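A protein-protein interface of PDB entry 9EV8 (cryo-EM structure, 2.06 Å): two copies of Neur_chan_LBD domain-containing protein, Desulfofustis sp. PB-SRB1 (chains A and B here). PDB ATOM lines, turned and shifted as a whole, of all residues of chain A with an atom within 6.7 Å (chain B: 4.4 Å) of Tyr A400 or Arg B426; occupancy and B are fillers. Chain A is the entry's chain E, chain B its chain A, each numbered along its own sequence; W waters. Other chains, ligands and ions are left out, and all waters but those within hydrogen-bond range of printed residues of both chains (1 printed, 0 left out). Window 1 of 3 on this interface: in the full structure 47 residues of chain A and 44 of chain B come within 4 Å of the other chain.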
ATOM      1  N   SER A 398      26.955  30.931  -4.426  1.00  0.00           N
ATOM      2  CA  SER A 398      27.924  29.846  -4.468  1.00  0.00           C
ATOM      3  C   SER A 398      27.285  28.610  -5.087  1.00  0.00           C
ATOM      4  O   SER A 398      26.062  28.465  -5.116  1.00  0.00           O
ATOM      5  CB  SER A 398      28.461  29.512  -3.070  1.00  0.00           C
ATOM      6  OG  SER A 398      27.434  29.002  -2.241  1.00  0.00           O
ATOM      7  N   PHE A 399      28.136  27.712  -5.588  1.00  0.00           N
ATOM      8  CA  PHE A 399      27.697  26.401  -6.055  1.00  0.00           C
ATOM      9  C   PHE A 399      27.622  25.452  -4.863  1.00  0.00           C
ATOM     10  O   PHE A 399      28.571  25.363  -4.077  1.00  0.00           O
ATOM     11  CB  PHE A 399      28.648  25.856  -7.120  1.00  0.00           C
ATOM     12  CG  PHE A 399      28.563  26.566  -8.443  1.00  0.00           C
ATOM     13  CD1 PHE A 399      29.285  27.724  -8.673  1.00  0.00           C
ATOM     14  CD2 PHE A 399      27.779  26.060  -9.467  1.00  0.00           C
ATOM     15  CE1 PHE A 399      29.214  28.373  -9.894  1.00  0.00           C
ATOM     16  CE2 PHE A 399      27.708  26.704 -10.690  1.00  0.00           C
ATOM     17  CZ  PHE A 399      28.426  27.861 -10.903  1.00  0.00           C
ATOM     18  N   TYR A 400      26.496  24.750  -4.725  1.00  0.00           N
ATOM     19  CA  TYR A 400      26.253  23.972  -3.512  1.00  0.00           C
ATOM     20  C   TYR A 400      27.219  22.799  -3.380  1.00  0.00           C
ATOM     21  O   TYR A 400      27.745  22.540  -2.291  1.00  0.00           O
ATOM     22  CB  TYR A 400      24.807  23.477  -3.486  1.00  0.00           C
ATOM     23  CG  TYR A 400      24.426  22.786  -2.198  1.00  0.00           C
ATOM     24  CD1 TYR A 400      24.407  23.481  -0.998  1.00  0.00           C
ATOM     25  CD2 TYR A 400      24.079  21.443  -2.182  1.00  0.00           C
ATOM     26  CE1 TYR A 400      24.061  22.858   0.183  1.00  0.00           C
ATOM     27  CE2 TYR A 400      23.729  20.811  -1.006  1.00  0.00           C
ATOM     28  CZ  TYR A 400      23.722  21.525   0.174  1.00  0.00           C
ATOM     29  OH  TYR A 400      23.375  20.900   1.349  1.00  0.00           O
ATOM     30  N   ASN A 401      27.467  22.076  -4.472  1.00  0.00           N
ATOM     31  CA  ASN A 401      28.282  20.869  -4.438  1.00  0.00           C
ATOM     32  C   ASN A 401      29.664  21.067  -5.052  1.00  0.00           C
ATOM     33  O   ASN A 401      30.209  20.131  -5.643  1.00  0.00           O
ATOM     34  CB  ASN A 401      27.556  19.723  -5.145  1.00  0.00           C
ATOM     35  CG  ASN A 401      26.277  19.323  -4.440  1.00  0.00           C
ATOM     36  OD1 ASN A 401      26.293  18.503  -3.523  1.00  0.00           O
ATOM     37  ND2 ASN A 401      25.162  19.906  -4.861  1.00  0.00           N
ATOM     38  N   GLN A 402      30.240  22.258  -4.921  1.00  0.00           N
ATOM     39  CA  GLN A 402      31.526  22.540  -5.545  1.00  0.00           C
ATOM     40  C   GLN A 402      32.647  21.751  -4.874  1.00  0.00           C
ATOM     41  O   GLN A 402      32.757  21.720  -3.646  1.00  0.00           O
ATOM     42  CB  GLN A 402      31.821  24.037  -5.484  1.00  0.00           C
ATOM     43  CG  GLN A 402      33.167  24.433  -6.062  1.00  0.00           C
ATOM     44  CD  GLN A 402      33.320  25.932  -6.190  1.00  0.00           C
ATOM     45  OE1 GLN A 402      32.341  26.656  -6.354  1.00  0.00           O
ATOM     46  NE2 GLN A 402      34.557  26.409  -6.114  1.00  0.00           N
ATOM     47  N   LEU A 431      31.509  19.196  -9.726  1.00  0.00           N
ATOM     48  CA  LEU A 431      30.402  19.106  -8.782  1.00  0.00           C
ATOM     49  C   LEU A 431      30.227  17.674  -8.297  1.00  0.00           C
ATOM     50  O   LEU A 431      30.260  16.735  -9.098  1.00  0.00           O
ATOM     51  CB  LEU A 431      29.104  19.607  -9.420  1.00  0.00           C
ATOM     52  CG  LEU A 431      29.144  21.027  -9.985  1.00  0.00           C
ATOM     53  CD1 LEU A 431      27.826  21.381 -10.650  1.00  0.00           C
ATOM     54  CD2 LEU A 431      29.483  22.024  -8.887  1.00  0.00           C
ATOM     55  N   GLN A 432      30.038  17.515  -6.989  1.00  0.00           N
ATOM     56  CA  GLN A 432      29.746  16.208  -6.417  1.00  0.00           C
ATOM     57  C   GLN A 432      28.331  15.765  -6.769  1.00  0.00           C
ATOM     58  O   GLN A 432      27.412  16.583  -6.866  1.00  0.00           O
ATOM     59  CB  GLN A 432      29.921  16.242  -4.899  1.00  0.00           C
ATOM     60  CG  GLN A 432      31.309  16.656  -4.447  1.00  0.00           C
ATOM     61  CD  GLN A 432      31.439  16.718  -2.940  1.00  0.00           C
ATOM     62  OE1 GLN A 432      30.474  16.492  -2.212  1.00  0.00           O
ATOM     63  NE2 GLN A 432      32.639  17.030  -2.464  1.00  0.00           N
ATOM     64  N   LYS A 451      23.151  23.385  -8.917  1.00  0.00           N
ATOM     65  CA  LYS A 451      22.410  24.184  -7.946  1.00  0.00           C
ATOM     66  C   LYS A 451      23.181  25.461  -7.630  1.00  0.00           C
ATOM     67  O   LYS A 451      24.363  25.405  -7.278  1.00  0.00           O
ATOM     68  CB  LYS A 451      22.160  23.389  -6.664  1.00  0.00           C
ATOM     69  CG  LYS A 451      21.446  22.066  -6.869  1.00  0.00           C
ATOM     70  CD  LYS A 451      21.273  21.332  -5.549  1.00  0.00           C
ATOM     71  CE  LYS A 451      20.662  19.956  -5.748  1.00  0.00           C
ATOM     72  NZ  LYS A 451      19.311  20.030  -6.370  1.00  0.00           N
ATOM     73  N   VAL A 452      22.508  26.603  -7.753  1.00  0.00           N
ATOM     74  CA  VAL A 452      23.069  27.907  -7.411  1.00  0.00           C
ATOM     75  C   VAL A 452      22.253  28.481  -6.260  1.00  0.00           C
ATOM     76  O   VAL A 452      21.040  28.682  -6.392  1.00  0.00           O
ATOM     77  CB  VAL A 452      23.070  28.860  -8.617  1.00  0.00           C
ATOM     78  CG1 VAL A 452      23.719  30.184  -8.252  1.00  0.00           C
ATOM     79  CG2 VAL A 452      23.780  28.225  -9.798  1.00  0.00           C
ATOM     80  N   ASP A 453      22.913  28.747  -5.135  1.00  0.00           N
ATOM     81  CA  ASP A 453      22.259  29.248  -3.932  1.00  0.00           C
ATOM     82  C   ASP A 453      22.769  30.641  -3.597  1.00  0.00           C
ATOM     83  O   ASP A 453      23.980  30.884  -3.616  1.00  0.00           O
ATOM     84  CB  ASP A 453      22.503  28.314  -2.742  1.00  0.00           C
ATOM     85  CG  ASP A 453      21.921  26.932  -2.950  1.00  0.00           C
ATOM     86  OD1 ASP A 453      21.399  26.657  -4.049  1.00  0.00           O
ATOM     87  OD2 ASP A 453      21.989  26.116  -2.008  1.00  0.00           O
ATOM     88  N   ARG A 504      17.204  29.178  -4.250  1.00  0.00           N
ATOM     89  CA  ARG A 504      17.986  28.199  -4.990  1.00  0.00           C
ATOM     90  C   ARG A 504      17.503  28.122  -6.432  1.00  0.00           C
ATOM     91  O   ARG A 504      16.297  28.096  -6.688  1.00  0.00           O
ATOM     92  CB  ARG A 504      17.903  26.816  -4.332  1.00  0.00           C
ATOM     93  CG  ARG A 504      18.541  25.700  -5.142  1.00  0.00           C
ATOM     94  CD  ARG A 504      18.618  24.410  -4.346  1.00  0.00           C
ATOM     95  NE  ARG A 504      19.587  24.498  -3.261  1.00  0.00           N
ATOM     96  CZ  ARG A 504      19.833  23.528  -2.391  1.00  0.00           C
ATOM     97  NH1 ARG A 504      19.190  22.374  -2.444  1.00  0.00           N
ATOM     98  NH2 ARG A 504      20.746  23.720  -1.445  1.00  0.00           N
ATOM     99  N   GLY B 353      31.528  16.593   4.696  1.00  0.00           N
ATOM    100  CA  GLY B 353      30.626  16.696   5.826  1.00  0.00           C
ATOM    101  C   GLY B 353      30.403  18.125   6.269  1.00  0.00           C
ATOM    102  O   GLY B 353      30.782  19.078   5.587  1.00  0.00           O
ATOM    103  N   THR B 354      29.768  18.258   7.438  1.00  0.00           N
ATOM    104  CA  THR B 354      29.372  19.541   8.010  1.00  0.00           C
ATOM    105  C   THR B 354      29.752  19.595   9.486  1.00  0.00           C
ATOM    106  O   THR B 354      29.636  18.593  10.198  1.00  0.00           O
ATOM    107  CB  THR B 354      27.860  19.772   7.854  1.00  0.00           C
ATOM    108  OG1 THR B 354      27.483  19.574   6.487  1.00  0.00           O
ATOM    109  CG2 THR B 354      27.483  21.182   8.269  1.00  0.00           C
ATOM    110  N   TRP B 407      39.183  22.353   1.672  1.00  0.00           N
ATOM    111  CA  TRP B 407      38.204  23.131   0.923  1.00  0.00           C
ATOM    112  C   TRP B 407      36.987  23.405   1.798  1.00  0.00           C
ATOM    113  O   TRP B 407      36.436  22.487   2.410  1.00  0.00           O
ATOM    114  CB  TRP B 407      37.798  22.391  -0.352  1.00  0.00           C
ATOM    115  CG  TRP B 407      36.595  22.968  -1.032  1.00  0.00           C
ATOM    116  CD1 TRP B 407      35.349  22.417  -1.095  1.00  0.00           C
ATOM    117  CD2 TRP B 407      36.519  24.211  -1.741  1.00  0.00           C
ATOM    118  NE1 TRP B 407      34.503  23.237  -1.800  1.00  0.00           N
ATOM    119  CE2 TRP B 407      35.197  24.346  -2.208  1.00  0.00           C
ATOM    120  CE3 TRP B 407      37.441  25.225  -2.026  1.00  0.00           C
ATOM    121  CZ2 TRP B 407      34.773  25.449  -2.945  1.00  0.00           C
ATOM    122  CZ3 TRP B 407      37.017  26.320  -2.758  1.00  0.00           C
ATOM    123  CH2 TRP B 407      35.696  26.423  -3.208  1.00  0.00           C
ATOM    124  N   SER B 408      36.569  24.672   1.852  1.00  0.00           N
ATOM    125  CA  SER B 408      35.499  25.106   2.742  1.00  0.00           C
ATOM    126  C   SER B 408      34.467  25.922   1.978  1.00  0.00           C
ATOM    127  O   SER B 408      34.816  26.720   1.103  1.00  0.00           O
ATOM    128  CB  SER B 408      36.047  25.938   3.907  1.00  0.00           C
ATOM    129  OG  SER B 408      37.006  25.210   4.651  1.00  0.00           O
ATOM    130  N   GLN B 409      33.195  25.716   2.316  1.00  0.00           N
ATOM    131  CA  GLN B 409      32.088  26.463   1.738  1.00  0.00           C
ATOM    132  C   GLN B 409      31.124  26.890   2.837  1.00  0.00           C
ATOM    133  O   GLN B 409      31.027  26.254   3.889  1.00  0.00           O
ATOM    134  CB  GLN B 409      31.339  25.638   0.684  1.00  0.00           C
ATOM    135  CG  GLN B 409      32.136  25.359  -0.573  1.00  0.00           C
ATOM    136  CD  GLN B 409      31.341  24.585  -1.606  1.00  0.00           C
ATOM    137  OE1 GLN B 409      31.211  25.012  -2.752  1.00  0.00           O
ATOM    138  NE2 GLN B 409      30.807  23.437  -1.203  1.00  0.00           N
ATOM    139  N   ASN B 410      30.408  27.986   2.571  1.00  0.00           N
ATOM    140  CA  ASN B 410      29.367  28.507   3.460  1.00  0.00           C
ATOM    141  C   ASN B 410      29.896  28.811   4.861  1.00  0.00           C
ATOM    142  O   ASN B 410      29.215  28.567   5.860  1.00  0.00           O
ATOM    143  CB  ASN B 410      28.176  27.546   3.538  1.00  0.00           C
ATOM    144  CG  ASN B 410      27.565  27.261   2.177  1.00  0.00           C
ATOM    145  OD1 ASN B 410      27.973  26.331   1.483  1.00  0.00           O
ATOM    146  ND2 ASN B 410      26.583  28.064   1.791  1.00  0.00           N
ATOM    147  N   PHE B 424      29.597  27.799  11.487  1.00  0.00           N
ATOM    148  CA  PHE B 424      29.097  26.815  10.536  1.00  0.00           C
ATOM    149  C   PHE B 424      30.082  26.671   9.385  1.00  0.00           C
ATOM    150  O   PHE B 424      30.664  27.661   8.934  1.00  0.00           O
ATOM    151  CB  PHE B 424      27.715  27.211  10.003  1.00  0.00           C
ATOM    152  CG  PHE B 424      27.106  26.201   9.075  1.00  0.00           C
ATOM    153  CD1 PHE B 424      26.351  25.156   9.572  1.00  0.00           C
ATOM    154  CD2 PHE B 424      27.288  26.298   7.705  1.00  0.00           C
ATOM    155  CE1 PHE B 424      25.788  24.224   8.722  1.00  0.00           C
ATOM    156  CE2 PHE B 424      26.729  25.368   6.851  1.00  0.00           C
ATOM    157  CZ  PHE B 424      25.980  24.331   7.360  1.00  0.00           C
ATOM    158  N   GLU B 425      30.265  25.438   8.911  1.00  0.00           N
ATOM    159  CA  GLU B 425      31.200  25.165   7.827  1.00  0.00           C
ATOM    160  C   GLU B 425      30.821  23.873   7.113  1.00  0.00           C
ATOM    161  O   GLU B 425      30.386  22.909   7.748  1.00  0.00           O
ATOM    162  CB  GLU B 425      32.636  25.067   8.356  1.00  0.00           C
ATOM    163  CG  GLU B 425      33.682  24.789   7.292  1.00  0.00           C
ATOM    164  CD  GLU B 425      35.048  24.506   7.883  1.00  0.00           C
ATOM    165  OE1 GLU B 425      35.208  24.652   9.112  1.00  0.00           O
ATOM    166  OE2 GLU B 425      35.963  24.134   7.119  1.00  0.00           O
ATOM    167  N   ARG B 426      30.985  23.870   5.791  1.00  0.00           N
ATOM    168  CA  ARG B 426      30.909  22.664   4.973  1.00  0.00           C
ATOM    169  C   ARG B 426      32.300  22.387   4.412  1.00  0.00           C
ATOM    170  O   ARG B 426      32.899  23.262   3.780  1.00  0.00           O
ATOM    171  CB  ARG B 426      29.892  22.830   3.843  1.00  0.00           C
ATOM    172  CG  ARG B 426      28.444  22.668   4.278  1.00  0.00           C
ATOM    173  CD  ARG B 426      27.486  23.384   3.336  1.00  0.00           C
ATOM    174  NE  ARG B 426      27.738  23.059   1.938  1.00  0.00           N
ATOM    175  CZ  ARG B 426      27.140  22.081   1.274  1.00  0.00           C
ATOM    176  NH1 ARG B 426      26.242  21.301   1.851  1.00  0.00           N
ATOM    177  NH2 ARG B 426      27.453  21.878  -0.004  1.00  0.00           N
ATOM    178  N   PHE B 427      32.811  21.180   4.644  1.00  0.00           N
ATOM    179  CA  PHE B 427      34.210  20.876   4.384  1.00  0.00           C
ATOM    180  C   PHE B 427      34.371  19.641   3.508  1.00  0.00           C
ATOM    181  O   PHE B 427      33.536  18.733   3.516  1.00  0.00           O
ATOM    182  CB  PHE B 427      34.981  20.668   5.699  1.00  0.00           C
ATOM    183  CG  PHE B 427      34.465  19.529   6.538  1.00  0.00           C
ATOM    184  CD1 PHE B 427      34.941  18.241   6.355  1.00  0.00           C
ATOM    185  CD2 PHE B 427      33.513  19.750   7.516  1.00  0.00           C
ATOM    186  CE1 PHE B 427      34.468  17.196   7.124  1.00  0.00           C
ATOM    187  CE2 PHE B 427      33.040  18.709   8.289  1.00  0.00           C
ATOM    188  CZ  PHE B 427      33.518  17.432   8.092  1.00  0.00           C
HETATM  189  O   HOH W   1      30.815  27.756  -4.798  1.00  0.00           O
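NE1 of Trp B407 lies within hydrogen-bond range of O of Gln A402, 3.0 Å away.
OE1 of Gln B409 lies close to O of Phe A399 (3.0 Å).
The side-chain hydroxyl (OH) of Tyr A400 sits at hydrogen-bond distance from the guanidinium group (NH1) of Arg B426, at 2.9 Å.
The side-chain amide nitrogen (NE2) of Gln B409 sits at hydrogen-bond distance from the backbone carbonyl oxygen (O) of Tyr A400, at 3.4 Å.
The backbone NH of Gln B409 is in hydrogen-bond range of the backbone carbonyl oxygen of Arg B426 (2.9 Å).
N of Tyr A400 is in hydrogen-bond range of O of Lys A451 (3.4 Å).
The side-chain amide oxygen (OD1) of Asn B410 sits at hydrogen-bond distance from the guanidinium group (NE) of Arg B426.
CB of Gln A402 touches OE1 of Gln B409 (3.0 Å).
Of chain B, only Gln B409 and Arg B426 come within 4 Å of Tyr A400.
Arg B426 touches just one residue of chain A: Tyr A400.
Of the printed residues of chain A, Trp B407 touches Gln A402 (3.0 Å).
Of the printed residues of chain B, Gln A402 touches Trp B407 and Gln B409.
Glu B425 touches none of the printed residues of chain A.
The nearest printed residue of chain B that does not touch Tyr A400 is Asn B410 (5.2 Å).
The nearest printed residue of chain A that does not touch Gln B409 is Asn A401 (4.7 Å).
Of the 11 printed residues of chain A, 3 touch a printed residue of chain B.
Hydrophobic or aromatic side chains of chain A within 4 Å of the printed part of chain B: Tyr A400.
Of the 10 printed residues of chain B, 3 touch a printed residue of chain A.
Hydrophobic or aromatic side chains of chain B that line the printed part of chain A: Trp B407.
Among the printed residues, no Asp or Glu carboxylate lies within 4 Å of a Lys or Arg side-chain nitrogen of the other chain.
No position is printed for both chains.
Of the 5 pairs that touch across the chains among the printed residues, none has its exchanged pair printed and touching as well.
Water W1 lies within hydrogen-bond range of OE1 of Gln A402 (2.4 Å), N of Phe A399 (2.8 Å) and OE1 of Gln B409 (3.4 Å).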
